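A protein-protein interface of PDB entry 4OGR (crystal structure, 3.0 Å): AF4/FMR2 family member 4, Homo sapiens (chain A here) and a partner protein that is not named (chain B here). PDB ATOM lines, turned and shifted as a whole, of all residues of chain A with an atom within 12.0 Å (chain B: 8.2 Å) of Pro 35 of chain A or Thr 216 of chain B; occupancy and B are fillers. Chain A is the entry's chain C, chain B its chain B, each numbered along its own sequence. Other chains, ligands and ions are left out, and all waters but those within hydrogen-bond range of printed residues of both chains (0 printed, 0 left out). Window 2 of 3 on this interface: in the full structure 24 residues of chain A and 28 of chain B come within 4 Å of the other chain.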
ATOM      1  N   PRO A  35      -0.963  18.240  -6.827  1.00  0.00           N
ATOM      2  CA  PRO A  35      -1.398  17.593  -5.584  1.00  0.00           C
ATOM      3  C   PRO A  35      -2.845  17.109  -5.659  1.00  0.00           C
ATOM      4  O   PRO A  35      -3.762  17.924  -5.768  1.00  0.00           O
ATOM      5  CB  PRO A  35      -1.238  18.702  -4.543  1.00  0.00           C
ATOM      6  CG  PRO A  35      -1.448  19.961  -5.311  1.00  0.00           C
ATOM      7  CD  PRO A  35      -0.913  19.707  -6.699  1.00  0.00           C
ATOM      8  N   LEU A  36      -3.038  15.794  -5.606  1.00  0.00           N
ATOM      9  CA  LEU A  36      -4.368  15.199  -5.726  1.00  0.00           C
ATOM     10  C   LEU A  36      -5.034  14.989  -4.373  1.00  0.00           C
ATOM     11  O   LEU A  36      -6.261  14.948  -4.277  1.00  0.00           O
ATOM     12  CB  LEU A  36      -4.290  13.852  -6.452  1.00  0.00           C
ATOM     13  CG  LEU A  36      -4.009  13.842  -7.954  1.00  0.00           C
ATOM     14  CD1 LEU A  36      -4.041  12.411  -8.452  1.00  0.00           C
ATOM     15  CD2 LEU A  36      -5.007  14.693  -8.723  1.00  0.00           C
ATOM     16  N   PHE A  37      -4.216  14.847  -3.334  1.00  0.00           N
ATOM     17  CA  PHE A  37      -4.713  14.502  -2.009  1.00  0.00           C
ATOM     18  C   PHE A  37      -4.276  15.498  -0.950  1.00  0.00           C
ATOM     19  O   PHE A  37      -3.161  16.016  -0.990  1.00  0.00           O
ATOM     20  CB  PHE A  37      -4.230  13.105  -1.632  1.00  0.00           C
ATOM     21  CG  PHE A  37      -5.007  12.006  -2.287  1.00  0.00           C
ATOM     22  CD1 PHE A  37      -6.232  11.608  -1.780  1.00  0.00           C
ATOM     23  CD2 PHE A  37      -4.519  11.380  -3.421  1.00  0.00           C
ATOM     24  CE1 PHE A  37      -6.952  10.600  -2.387  1.00  0.00           C
ATOM     25  CE2 PHE A  37      -5.233  10.373  -4.032  1.00  0.00           C
ATOM     26  CZ  PHE A  37      -6.452   9.982  -3.516  1.00  0.00           C
ATOM     27  N   ALA A  38      -5.175  15.776  -0.012  1.00  0.00           N
ATOM     28  CA  ALA A  38      -4.835  16.575   1.152  1.00  0.00           C
ATOM     29  C   ALA A  38      -3.974  15.756   2.098  1.00  0.00           C
ATOM     30  O   ALA A  38      -3.927  14.528   2.016  1.00  0.00           O
ATOM     31  CB  ALA A  38      -6.088  17.060   1.855  1.00  0.00           C
ATOM     32  N   GLU A  39      -3.296  16.445   3.002  1.00  0.00           N
ATOM     33  CA  GLU A  39      -2.430  15.786   3.960  1.00  0.00           C
ATOM     34  C   GLU A  39      -3.294  15.007   4.962  1.00  0.00           C
ATOM     35  O   GLU A  39      -4.210  15.577   5.560  1.00  0.00           O
ATOM     36  CB  GLU A  39      -1.554  16.823   4.658  1.00  0.00           C
ATOM     37  CG  GLU A  39      -0.489  16.254   5.564  1.00  0.00           C
ATOM     38  CD  GLU A  39       0.460  17.328   6.060  1.00  0.00           C
ATOM     39  OE1 GLU A  39       0.432  17.641   7.273  1.00  0.00           O
ATOM     40  OE2 GLU A  39       1.234  17.860   5.232  1.00  0.00           O
ATOM     41  N   PRO A  40      -3.026  13.698   5.134  1.00  0.00           N
ATOM     42  CA  PRO A  40      -3.906  12.885   5.988  1.00  0.00           C
ATOM     43  C   PRO A  40      -3.957  13.365   7.439  1.00  0.00           C
ATOM     44  O   PRO A  40      -2.966  13.889   7.949  1.00  0.00           O
ATOM     45  CB  PRO A  40      -3.288  11.483   5.902  1.00  0.00           C
ATOM     46  CG  PRO A  40      -2.434  11.501   4.687  1.00  0.00           C
ATOM     47  CD  PRO A  40      -1.928  12.896   4.568  1.00  0.00           C
ATOM     48  N   TYR A  41      -5.104  13.174   8.085  1.00  0.00           N
ATOM     49  CA  TYR A  41      -5.350  13.706   9.424  1.00  0.00           C
ATOM     50  C   TYR A  41      -5.829  12.625  10.392  1.00  0.00           C
ATOM     51  O   TYR A  41      -6.388  11.609   9.978  1.00  0.00           O
ATOM     52  CB  TYR A  41      -6.383  14.828   9.344  1.00  0.00           C
ATOM     53  CG  TYR A  41      -7.603  14.434   8.550  1.00  0.00           C
ATOM     54  CD1 TYR A  41      -8.661  13.773   9.153  1.00  0.00           C
ATOM     55  CD2 TYR A  41      -7.687  14.704   7.192  1.00  0.00           C
ATOM     56  CE1 TYR A  41      -9.776  13.403   8.429  1.00  0.00           C
ATOM     57  CE2 TYR A  41      -8.796  14.337   6.459  1.00  0.00           C
ATOM     58  CZ  TYR A  41      -9.837  13.685   7.082  1.00  0.00           C
ATOM     59  OH  TYR A  41     -10.945  13.315   6.357  1.00  0.00           O
ATOM     60  N   LEU B 163       1.741   9.399  -3.112  1.00  0.00           N
ATOM     61  CA  LEU B 163       0.626  10.097  -3.737  1.00  0.00           C
ATOM     62  C   LEU B 163      -0.269  10.758  -2.693  1.00  0.00           C
ATOM     63  O   LEU B 163      -0.658  11.917  -2.843  1.00  0.00           O
ATOM     64  CB  LEU B 163      -0.196   9.129  -4.593  1.00  0.00           C
ATOM     65  CG  LEU B 163      -1.384   9.736  -5.344  1.00  0.00           C
ATOM     66  CD1 LEU B 163      -0.893  10.650  -6.446  1.00  0.00           C
ATOM     67  CD2 LEU B 163      -2.289   8.649  -5.908  1.00  0.00           C
ATOM     68  N   ARG B 165       0.480  11.527   0.312  1.00  0.00           N
ATOM     69  CA  ARG B 165       1.239  12.391   1.217  1.00  0.00           C
ATOM     70  C   ARG B 165       1.214  11.872   2.656  1.00  0.00           C
ATOM     71  O   ARG B 165       0.984  12.629   3.601  1.00  0.00           O
ATOM     72  CB  ARG B 165       0.691  13.821   1.166  1.00  0.00           C
ATOM     73  CG  ARG B 165       0.587  14.381  -0.239  1.00  0.00           C
ATOM     74  CD  ARG B 165      -0.221  15.660  -0.276  1.00  0.00           C
ATOM     75  NE  ARG B 165       0.429  16.771   0.409  1.00  0.00           N
ATOM     76  CZ  ARG B 165      -0.188  17.906   0.728  1.00  0.00           C
ATOM     77  NH1 ARG B 165      -1.466  18.076   0.417  1.00  0.00           N
ATOM     78  NH2 ARG B 165       0.468  18.873   1.354  1.00  0.00           N
ATOM     79  N   PRO B 213      -8.175  11.270   2.898  1.00  0.00           N
ATOM     80  CA  PRO B 213      -9.437  11.779   2.357  1.00  0.00           C
ATOM     81  C   PRO B 213      -9.660  11.361   0.907  1.00  0.00           C
ATOM     82  O   PRO B 213      -8.884  10.583   0.345  1.00  0.00           O
ATOM     83  CB  PRO B 213      -9.288  13.305   2.468  1.00  0.00           C
ATOM     84  CG  PRO B 213      -7.873  13.566   2.917  1.00  0.00           C
ATOM     85  CD  PRO B 213      -7.113  12.285   2.831  1.00  0.00           C
ATOM     86  N   VAL B 214     -10.717  11.896   0.308  1.00  0.00           N
ATOM     87  CA  VAL B 214     -10.980  11.700  -1.107  1.00  0.00           C
ATOM     88  C   VAL B 214     -10.182  12.731  -1.901  1.00  0.00           C
ATOM     89  O   VAL B 214      -9.910  13.827  -1.409  1.00  0.00           O
ATOM     90  CB  VAL B 214     -12.489  11.815  -1.404  1.00  0.00           C
ATOM     91  CG1 VAL B 214     -12.747  11.973  -2.885  1.00  0.00           C
ATOM     92  CG2 VAL B 214     -13.225  10.601  -0.867  1.00  0.00           C
ATOM     93  N   SER B 215      -9.802  12.374  -3.125  1.00  0.00           N
ATOM     94  CA  SER B 215      -8.960  13.236  -3.953  1.00  0.00           C
ATOM     95  C   SER B 215      -9.685  14.501  -4.390  1.00  0.00           C
ATOM     96  O   SER B 215     -10.886  14.648  -4.178  1.00  0.00           O
ATOM     97  CB  SER B 215      -8.480  12.483  -5.192  1.00  0.00           C
ATOM     98  OG  SER B 215      -9.560  12.229  -6.074  1.00  0.00           O
ATOM     99  N   THR B 216      -8.940  15.408  -5.012  1.00  0.00           N
ATOM    100  CA  THR B 216      -9.510  16.641  -5.538  1.00  0.00           C
ATOM    101  C   THR B 216     -10.533  16.371  -6.639  1.00  0.00           C
ATOM    102  O   THR B 216     -11.345  17.239  -6.961  1.00  0.00           O
ATOM    103  CB  THR B 216      -8.413  17.558  -6.097  1.00  0.00           C
ATOM    104  OG1 THR B 216      -7.652  16.847  -7.080  1.00  0.00           O
ATOM    105  CG2 THR B 216      -7.481  18.024  -4.989  1.00  0.00           C
ATOM    106  N   ASP B 217     -10.486  15.168  -7.208  1.00  0.00           N
ATOM    107  CA  ASP B 217     -11.411  14.770  -8.269  1.00  0.00           C
ATOM    108  C   ASP B 217     -12.447  13.764  -7.761  1.00  0.00           C
ATOM    109  O   ASP B 217     -13.097  13.075  -8.546  1.00  0.00           O
ATOM    110  CB  ASP B 217     -10.643  14.191  -9.462  1.00  0.00           C
ATOM    111  CG  ASP B 217     -10.009  15.269 -10.325  1.00  0.00           C
ATOM    112  OD1 ASP B 217      -9.883  16.422  -9.857  1.00  0.00           O
ATOM    113  OD2 ASP B 217      -9.644  14.965 -11.481  1.00  0.00           O
ATOM    114  N   GLY B 218     -12.592  13.684  -6.442  1.00  0.00           N
ATOM    115  CA  GLY B 218     -13.699  12.962  -5.837  1.00  0.00           C
ATOM    116  C   GLY B 218     -13.584  11.450  -5.780  1.00  0.00           C
ATOM    117  O   GLY B 218     -14.593  10.771  -5.590  1.00  0.00           O
ATOM    118  N   LYS B 219     -12.374  10.919  -5.934  1.00  0.00           N
ATOM    119  CA  LYS B 219     -12.159   9.470  -5.898  1.00  0.00           C
ATOM    120  C   LYS B 219     -11.305   9.015  -4.714  1.00  0.00           C
ATOM    121  O   LYS B 219     -10.336   9.673  -4.334  1.00  0.00           O
ATOM    122  CB  LYS B 219     -11.527   8.983  -7.203  1.00  0.00           C
ATOM    123  CG  LYS B 219     -12.513   8.924  -8.356  1.00  0.00           C
ATOM    124  CD  LYS B 219     -11.865   8.418  -9.628  1.00  0.00           C
ATOM    125  CE  LYS B 219     -12.898   8.229 -10.724  1.00  0.00           C
ATOM    126  NZ  LYS B 219     -12.290   7.687 -11.967  1.00  0.00           N
ATOM    127  N   HIS B 220     -11.689   7.877  -4.141  1.00  0.00           N
ATOM    128  CA  HIS B 220     -10.967   7.267  -3.030  1.00  0.00           C
ATOM    129  C   HIS B 220      -9.539   6.923  -3.429  1.00  0.00           C
ATOM    130  O   HIS B 220      -9.246   6.744  -4.609  1.00  0.00           O
ATOM    131  CB  HIS B 220     -11.692   6.007  -2.559  1.00  0.00           C
ATOM    132  CG  HIS B 220     -13.102   6.253  -2.125  1.00  0.00           C
ATOM    133  ND1 HIS B 220     -13.423   7.083  -1.074  1.00  0.00           N
ATOM    134  CD2 HIS B 220     -14.277   5.782  -2.606  1.00  0.00           C
ATOM    135  CE1 HIS B 220     -14.735   7.112  -0.922  1.00  0.00           C
ATOM    136  NE2 HIS B 220     -15.276   6.330  -1.839  1.00  0.00           N
ATOM    137  N   TYR B 224      -6.776   4.907  -7.202  1.00  0.00           N
ATOM    138  CA  TYR B 224      -5.541   5.280  -7.887  1.00  0.00           C
ATOM    139  C   TYR B 224      -4.507   4.158  -7.812  1.00  0.00           C
ATOM    140  O   TYR B 224      -3.364   4.334  -8.233  1.00  0.00           O
ATOM    141  CB  TYR B 224      -4.962   6.564  -7.291  1.00  0.00           C
ATOM    142  CG  TYR B 224      -5.856   7.768  -7.464  1.00  0.00           C
ATOM    143  CD1 TYR B 224      -6.925   7.989  -6.605  1.00  0.00           C
ATOM    144  CD2 TYR B 224      -5.641   8.676  -8.491  1.00  0.00           C
ATOM    145  CE1 TYR B 224      -7.750   9.087  -6.759  1.00  0.00           C
ATOM    146  CE2 TYR B 224      -6.461   9.778  -8.653  1.00  0.00           C
ATOM    147  CZ  TYR B 224      -7.513   9.977  -7.786  1.00  0.00           C
ATOM    148  OH  TYR B 224      -8.334  11.067  -7.941  1.00  0.00           O
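Pro 35 of chain A touches one residue of chain B.
Thr 216 of chain B touches just these residues of chain A: Pro 35 and Leu 36.
Val 214 of chain B touches one residue of chain A.
No residue of chain A comes within 4 Å of Asp 217 of chain B.
Of the printed residues of chain B, Ala 38 of chain A touches Arg 165 and Pro 213.
Printed residues of chain A within 4 Å of Lys 219 of chain B: Phe 37 (3.98 Å).
Printed residues of chain A within 4 Å of Pro 213 of chain B: Phe 37, Ala 38 and Tyr 41.
Of the printed residues of chain A, Tyr 224 of chain B touches Leu 36 and Phe 37.
His 220 of chain B touches none of the printed residues of chain A.
The nearest printed residue of chain A that does not touch Lys 219 of chain B is Leu 36 of chain A (6.7 Å).
Among the printed residues, pairs that only touch across the chains: Pro 35 of chain A with Thr 216 of chain B (3.8 Å), Leu 36 of chain A with Ser 215 of chain B (3.2 Å), Leu 36 of chain A with Tyr 224 of chain B (3.6 Å), Phe 37 of chain A with Leu 163 of chain B (3.9 Å), Phe 37 of chain A with Pro 213 of chain B (3.3 Å), Phe 37 of chain A with Val 214 of chain B (3.9 Å), Phe 37 of chain A with Ser 215 of chain B (3.4 Å), Phe 37 of chain A with Lys 219 of chain B (3.98 Å), Phe 37 of chain A with Tyr 224 of chain B (3.6 Å), Ala 38 of chain A with Arg 165 of chain B (3.8 Å), Ala 38 of chain A with Pro 213 of chain B (3.98 Å), Glu 39 of chain A with Arg 165 of chain B (3.6 Å), Pro 40 of chain A with Arg 165 of chain B (3.1 Å) and Tyr 41 of chain A with Pro 213 of chain B (3.7 Å).
The backbone carbonyl oxygen (O) of Phe 37 of chain A sits at hydrogen-bond distance from the guanidinium group (NH1) of Arg 165 of chain B (3.0 Å).
The backbone NH (N) of Thr 216 of chain B sits at hydrogen-bond distance from the backbone carbonyl oxygen (O) of Leu 36 of chain A (2.8 Å).
Along chain A the printed residues that touch a printed residue of chain B span positions 35 to 41.
Of the 11 printed residues of chain B, 8 touch a printed residue of chain A.
Hydrophobic or aromatic side chains of chain B that line the printed part of chain A: Leu 163, Pro 213 and Tyr 224.
Among the printed residues, 16 pairs touch across the chains.
The side-chain hydroxyl (OG) of Ser 215 of chain B lies close to the backbone NH (N) of Asp 217 of chain B.
The side-chain hydroxyl (OG) of Ser 215 of chain B is in hydrogen-bond range of the backbone NH (N) of Gly 218 of chain B.
N of Lys 219 of chain B sits at hydrogen-bond distance from OG of Ser 215 of chain B, at 3.1 Å.
OG of Ser 215 of chain B is in hydrogen-bond range of OH of Tyr 224 of chain B (2.5 Å).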
